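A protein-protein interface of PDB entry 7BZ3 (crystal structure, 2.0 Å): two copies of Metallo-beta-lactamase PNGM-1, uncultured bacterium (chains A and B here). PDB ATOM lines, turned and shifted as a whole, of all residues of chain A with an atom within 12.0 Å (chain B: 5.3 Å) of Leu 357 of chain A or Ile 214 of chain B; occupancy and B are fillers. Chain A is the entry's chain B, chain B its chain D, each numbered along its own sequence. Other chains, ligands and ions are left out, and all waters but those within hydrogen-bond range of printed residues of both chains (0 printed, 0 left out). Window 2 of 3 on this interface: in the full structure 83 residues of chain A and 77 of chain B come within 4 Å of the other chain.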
ATOM      1  N   TYR A 348      10.477 -22.922  32.645  1.00  0.00           N
ATOM      2  CA  TYR A 348      11.932 -22.678  32.821  1.00  0.00           C
ATOM      3  C   TYR A 348      12.185 -22.243  34.259  1.00  0.00           C
ATOM      4  O   TYR A 348      11.365 -21.471  34.813  1.00  0.00           O
ATOM      5  CB  TYR A 348      12.473 -21.556  31.944  1.00  0.00           C
ATOM      6  CG  TYR A 348      12.575 -21.850  30.474  1.00  0.00           C
ATOM      7  CD1 TYR A 348      13.446 -22.814  29.985  1.00  0.00           C
ATOM      8  CD2 TYR A 348      11.820 -21.136  29.557  1.00  0.00           C
ATOM      9  CE1 TYR A 348      13.520 -23.099  28.627  1.00  0.00           C
ATOM     10  CE2 TYR A 348      11.891 -21.401  28.200  1.00  0.00           C
ATOM     11  CZ  TYR A 348      12.763 -22.364  27.729  1.00  0.00           C
ATOM     12  OH  TYR A 348      12.827 -22.615  26.393  1.00  0.00           O
ATOM     13  N   GLN A 350      15.284 -20.242  36.604  1.00  0.00           N
ATOM     14  CA  GLN A 350      16.385 -19.262  36.404  1.00  0.00           C
ATOM     15  C   GLN A 350      17.704 -20.031  36.272  1.00  0.00           C
ATOM     16  O   GLN A 350      18.566 -19.557  35.521  1.00  0.00           O
ATOM     17  CB  GLN A 350      16.374 -18.198  37.505  1.00  0.00           C
ATOM     18  CG  GLN A 350      17.218 -16.969  37.173  1.00  0.00           C
ATOM     19  CD  GLN A 350      16.714 -16.220  35.964  1.00  0.00           C
ATOM     20  OE1 GLN A 350      15.610 -15.685  35.950  1.00  0.00           O
ATOM     21  NE2 GLN A 350      17.541 -16.157  34.934  1.00  0.00           N
ATOM     22  N   TYR A 351      17.805 -21.221  36.880  1.00  0.00           N
ATOM     23  CA  TYR A 351      18.985 -22.132  36.777  1.00  0.00           C
ATOM     24  C   TYR A 351      19.264 -22.458  35.301  1.00  0.00           C
ATOM     25  O   TYR A 351      20.413 -22.402  34.877  1.00  0.00           O
ATOM     26  CB  TYR A 351      18.794 -23.392  37.634  1.00  0.00           C
ATOM     27  CG  TYR A 351      19.903 -24.405  37.490  1.00  0.00           C
ATOM     28  CD1 TYR A 351      21.179 -24.139  37.969  1.00  0.00           C
ATOM     29  CD2 TYR A 351      19.687 -25.627  36.861  1.00  0.00           C
ATOM     30  CE1 TYR A 351      22.214 -25.051  37.813  1.00  0.00           C
ATOM     31  CE2 TYR A 351      20.716 -26.541  36.682  1.00  0.00           C
ATOM     32  CZ  TYR A 351      21.986 -26.264  37.180  1.00  0.00           C
ATOM     33  OH  TYR A 351      23.002 -27.176  37.051  1.00  0.00           O
ATOM     34  N   ILE A 352      18.238 -22.760  34.507  1.00  0.00           N
ATOM     35  CA  ILE A 352      18.422 -23.111  33.065  1.00  0.00           C
ATOM     36  C   ILE A 352      18.596 -21.822  32.259  1.00  0.00           C
ATOM     37  O   ILE A 352      19.414 -21.797  31.326  1.00  0.00           O
ATOM     38  CB  ILE A 352      17.286 -24.033  32.554  1.00  0.00           C
ATOM     39  CG1 ILE A 352      17.418 -25.444  33.143  1.00  0.00           C
ATOM     40  CG2 ILE A 352      17.231 -24.084  31.033  1.00  0.00           C
ATOM     41  CD1 ILE A 352      18.614 -26.249  32.626  1.00  0.00           C
ATOM     42  N   LEU A 353      17.916 -20.751  32.629  1.00  0.00           N
ATOM     43  CA  LEU A 353      17.965 -19.540  31.785  1.00  0.00           C
ATOM     44  C   LEU A 353      19.337 -18.894  31.938  1.00  0.00           C
ATOM     45  O   LEU A 353      19.763 -18.282  30.978  1.00  0.00           O
ATOM     46  CB  LEU A 353      16.789 -18.637  32.165  1.00  0.00           C
ATOM     47  CG  LEU A 353      15.419 -19.180  31.734  1.00  0.00           C
ATOM     48  CD1 LEU A 353      14.284 -18.231  32.123  1.00  0.00           C
ATOM     49  CD2 LEU A 353      15.357 -19.425  30.234  1.00  0.00           C
ATOM     50  N   ASP A 354      20.029 -19.130  33.056  1.00  0.00           N
ATOM     51  CA  ASP A 354      21.326 -18.487  33.385  1.00  0.00           C
ATOM     52  C   ASP A 354      22.406 -19.147  32.546  1.00  0.00           C
ATOM     53  O   ASP A 354      23.505 -18.624  32.518  1.00  0.00           O
ATOM     54  CB  ASP A 354      21.698 -18.616  34.869  1.00  0.00           C
ATOM     55  CG  ASP A 354      20.938 -17.695  35.806  1.00  0.00           C
ATOM     56  OD1 ASP A 354      20.492 -16.635  35.354  1.00  0.00           O
ATOM     57  OD2 ASP A 354      20.776 -18.074  36.977  1.00  0.00           O
ATOM     58  N   GLY A 355      22.089 -20.272  31.898  1.00  0.00           N
ATOM     59  CA  GLY A 355      23.046 -21.003  31.053  1.00  0.00           C
ATOM     60  C   GLY A 355      23.174 -20.397  29.663  1.00  0.00           C
ATOM     61  O   GLY A 355      24.071 -20.827  28.920  1.00  0.00           O
ATOM     62  N   ARG A 356      22.319 -19.443  29.285  1.00  0.00           N
ATOM     63  CA  ARG A 356      22.349 -18.871  27.911  1.00  0.00           C
ATOM     64  C   ARG A 356      23.760 -18.366  27.585  1.00  0.00           C
ATOM     65  O   ARG A 356      24.389 -17.788  28.484  1.00  0.00           O
ATOM     66  CB  ARG A 356      21.332 -17.741  27.736  1.00  0.00           C
ATOM     67  CG  ARG A 356      19.948 -18.217  27.326  1.00  0.00           C
ATOM     68  CD  ARG A 356      19.121 -17.134  26.665  1.00  0.00           C
ATOM     69  NE  ARG A 356      17.711 -17.405  26.905  1.00  0.00           N
ATOM     70  CZ  ARG A 356      17.004 -18.344  26.283  1.00  0.00           C
ATOM     71  NH1 ARG A 356      17.566 -19.089  25.341  1.00  0.00           N
ATOM     72  NH2 ARG A 356      15.724 -18.517  26.587  1.00  0.00           N
ATOM     73  N   LEU A 357      24.219 -18.633  26.356  1.00  0.00           N
ATOM     74  CA  LEU A 357      25.458 -18.111  25.718  1.00  0.00           C
ATOM     75  C   LEU A 357      25.139 -16.799  24.991  1.00  0.00           C
ATOM     76  O   LEU A 357      26.064 -16.184  24.482  1.00  0.00           O
ATOM     77  CB  LEU A 357      25.958 -19.139  24.704  1.00  0.00           C
ATOM     78  CG  LEU A 357      27.360 -18.885  24.156  1.00  0.00           C
ATOM     79  CD1 LEU A 357      28.408 -19.232  25.210  1.00  0.00           C
ATOM     80  CD2 LEU A 357      27.593 -19.650  22.854  1.00  0.00           C
ATOM     81  N   PRO B 212      21.825 -21.798  22.161  1.00  0.00           N
ATOM     82  CA  PRO B 212      23.220 -21.746  22.572  1.00  0.00           C
ATOM     83  C   PRO B 212      23.351 -21.665  24.100  1.00  0.00           C
ATOM     84  O   PRO B 212      22.767 -20.776  24.701  1.00  0.00           O
ATOM     85  CB  PRO B 212      23.678 -20.453  21.889  1.00  0.00           C
ATOM     86  CG  PRO B 212      22.877 -20.449  20.629  1.00  0.00           C
ATOM     87  CD  PRO B 212      21.504 -20.809  21.130  1.00  0.00           C
ATOM     88  N   ASN B 213      24.085 -22.594  24.691  1.00  0.00           N
ATOM     89  CA  ASN B 213      24.356 -22.616  26.149  1.00  0.00           C
ATOM     90  C   ASN B 213      25.862 -22.693  26.414  1.00  0.00           C
ATOM     91  O   ASN B 213      26.630 -23.100  25.532  1.00  0.00           O
ATOM     92  CB  ASN B 213      23.594 -23.747  26.824  1.00  0.00           C
ATOM     93  CG  ASN B 213      24.095 -25.104  26.399  1.00  0.00           C
ATOM     94  OD1 ASN B 213      25.193 -25.497  26.789  1.00  0.00           O
ATOM     95  ND2 ASN B 213      23.302 -25.832  25.632  1.00  0.00           N
ATOM     96  N   ILE B 214      26.250 -22.332  27.634  1.00  0.00           N
ATOM     97  CA  ILE B 214      27.666 -22.335  28.096  1.00  0.00           C
ATOM     98  C   ILE B 214      28.123 -23.768  28.380  1.00  0.00           C
ATOM     99  O   ILE B 214      29.337 -23.947  28.526  1.00  0.00           O
ATOM    100  CB  ILE B 214      27.840 -21.454  29.353  1.00  0.00           C
ATOM    101  CG1 ILE B 214      26.940 -21.896  30.512  1.00  0.00           C
ATOM    102  CG2 ILE B 214      27.639 -20.000  29.009  1.00  0.00           C
ATOM    103  CD1 ILE B 214      27.495 -21.594  31.874  1.00  0.00           C
ATOM    104  N   TRP B 215      27.212 -24.741  28.549  1.00  0.00           N
ATOM    105  CA  TRP B 215      27.617 -26.125  28.939  1.00  0.00           C
ATOM    106  C   TRP B 215      28.220 -26.887  27.754  1.00  0.00           C
ATOM    107  O   TRP B 215      29.344 -27.398  27.911  1.00  0.00           O
ATOM    108  CB  TRP B 215      26.468 -26.873  29.605  1.00  0.00           C
ATOM    109  CG  TRP B 215      26.017 -26.101  30.795  1.00  0.00           C
ATOM    110  CD1 TRP B 215      26.786 -25.736  31.863  1.00  0.00           C
ATOM    111  CD2 TRP B 215      24.723 -25.501  30.998  1.00  0.00           C
ATOM    112  NE1 TRP B 215      26.041 -24.997  32.744  1.00  0.00           N
ATOM    113  CE2 TRP B 215      24.778 -24.831  32.240  1.00  0.00           C
ATOM    114  CE3 TRP B 215      23.541 -25.470  30.261  1.00  0.00           C
ATOM    115  CZ2 TRP B 215      23.688 -24.152  32.759  1.00  0.00           C
ATOM    116  CZ3 TRP B 215      22.461 -24.795  30.772  1.00  0.00           C
ATOM    117  CH2 TRP B 215      22.540 -24.153  32.005  1.00  0.00           C
ATOM    118  N   TYR B 216      27.517 -26.925  26.621  1.00  0.00           N
ATOM    119  CA  TYR B 216      27.842 -27.782  25.452  1.00  0.00           C
ATOM    120  C   TYR B 216      29.271 -27.505  25.000  1.00  0.00           C
ATOM    121  O   TYR B 216      30.012 -28.448  24.756  1.00  0.00           O
ATOM    122  CB  TYR B 216      26.822 -27.616  24.315  1.00  0.00           C
ATOM    123  CG  TYR B 216      27.005 -28.592  23.178  1.00  0.00           C
ATOM    124  CD1 TYR B 216      28.079 -28.461  22.308  1.00  0.00           C
ATOM    125  CD2 TYR B 216      26.121 -29.654  22.956  1.00  0.00           C
ATOM    126  CE1 TYR B 216      28.314 -29.376  21.292  1.00  0.00           C
ATOM    127  CE2 TYR B 216      26.327 -30.551  21.916  1.00  0.00           C
ATOM    128  CZ  TYR B 216      27.423 -30.412  21.078  1.00  0.00           C
ATOM    129  OH  TYR B 216      27.656 -31.265  20.023  1.00  0.00           O
ATOM    130  N   PRO B 217      29.675 -26.218  24.835  1.00  0.00           N
ATOM    131  CA  PRO B 217      31.007 -25.875  24.329  1.00  0.00           C
ATOM    132  C   PRO B 217      32.134 -26.415  25.216  1.00  0.00           C
ATOM    133  O   PRO B 217      33.195 -26.784  24.673  1.00  0.00           O
ATOM    134  CB  PRO B 217      31.045 -24.337  24.314  1.00  0.00           C
ATOM    135  CG  PRO B 217      29.603 -23.902  24.331  1.00  0.00           C
ATOM    136  CD  PRO B 217      28.840 -25.017  25.025  1.00  0.00           C
ATOM    137  N   GLU B 218      31.872 -26.471  26.528  1.00  0.00           N
ATOM    138  CA  GLU B 218      32.825 -26.945  27.565  1.00  0.00           C
ATOM    139  C   GLU B 218      32.868 -28.475  27.568  1.00  0.00           C
ATOM    140  O   GLU B 218      33.988 -29.022  27.514  1.00  0.00           O
ATOM    141  CB  GLU B 218      32.441 -26.378  28.933  1.00  0.00           C
ATOM    142  CG  GLU B 218      33.158 -27.028  30.110  1.00  0.00           C
ATOM    143  CD  GLU B 218      34.666 -26.857  30.155  1.00  0.00           C
ATOM    144  OE1 GLU B 218      35.171 -26.335  31.175  1.00  0.00           O
ATOM    145  OE2 GLU B 218      35.344 -27.284  29.192  1.00  0.00           O
ATOM    146  N   ILE B 265      29.865 -22.325  18.059  1.00  0.00           N
ATOM    147  CA  ILE B 265      30.004 -23.404  19.078  1.00  0.00           C
ATOM    148  C   ILE B 265      31.106 -24.363  18.624  1.00  0.00           C
ATOM    149  O   ILE B 265      32.018 -24.566  19.390  1.00  0.00           O
ATOM    150  CB  ILE B 265      28.644 -24.078  19.310  1.00  0.00           C
ATOM    151  CG1 ILE B 265      27.728 -23.115  20.068  1.00  0.00           C
ATOM    152  CG2 ILE B 265      28.803 -25.428  19.995  1.00  0.00           C
ATOM    153  CD1 ILE B 265      26.256 -23.399  19.941  1.00  0.00           C
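The backbone NH (N) of Tyr 216 of chain B lies within hydrogen-bond range of the side-chain amide oxygen (OD1) of Asn 213 of chain B (2.7 Å).
The side-chain amide oxygen (OD1) of Asn 213 of chain B sits at hydrogen-bond distance from the backbone NH (N) of Trp 215 of chain B.
Trp 215 of chain B touches Tyr 351 of chain A (CH2 to O, 3.98 Å).
CH2 of Trp 215 of chain B touches O of Ile 352 of chain A, 3.97 Å away.
Asn 213 of chain B touches Gly 355 of chain A.
Trp 215 of chain B touches Gly 355 of chain A (CH2 to CA, 3.3 Å).
CA of Arg 356 of chain A touches O of Pro 212 of chain B, 3.8 Å away.
O of Arg 356 of chain A touches CG2 of Ile 214 of chain B (3.97 Å).
Asn 213 of chain B touches Leu 357 of chain A.
Ile 214 of chain B touches Leu 357 of chain A (CG2 to CD1, 3.95 Å).
No position is printed for both chains.
Of chain B, only Pro 212 (3.1 Å), Asn 213 (3.9 Å) and Ile 214 (3.95 Å) come within 4 Å of Leu 357 of chain A.
Printed residues of chain A within 4 Å of Ile 214 of chain B: Gly 355 (2.9 Å), Arg 356 (3.97 Å) and Leu 357 (3.95 Å).
Trp 215 of chain B touches just these residues of chain A: Tyr 351, Ile 352 and Gly 355.
No residue of chain A comes within 4 Å of Pro 217 of chain B.
No residue of chain A comes within 4 Å of Glu 218 of chain B.
No residue of chain A comes within 4 Å of Ile 265 of chain B.
Of the printed residues of chain B, Tyr 351 of chain A touches Trp 215.
Of the printed residues of chain B, Arg 356 of chain A touches Pro 212 and Ile 214.
Printed residues of chain B within 4 Å of Ile 352 of chain A: Trp 215.
Asp 354 of chain A touches none of the printed residues of chain B.
Printed residues of chain A that touch a printed residue of chain B: Tyr 351, Ile 352, Gly 355, Arg 356 and Leu 357.
Printed residues of chain B that touch a printed residue of chain A: Pro 212, Asn 213, Ile 214 and Trp 215.
Hydrophobic or aromatic side chains of chain B that line the printed part of chain A: Pro 212, Ile 214 and Trp 215.
Among the printed residues, no Asp or Glu carboxylate lies within 4 Å of a Lys or Arg side-chain nitrogen of the other chain.
O of Pro 212 of chain B lies within hydrogen-bond range of N of Leu 357 of chain A, at 3.1 Å.
The backbone NH (N) of Ile 214 of chain B sits at hydrogen-bond distance from the backbone carbonyl oxygen (O) of Gly 355 of chain A (2.9 Å).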
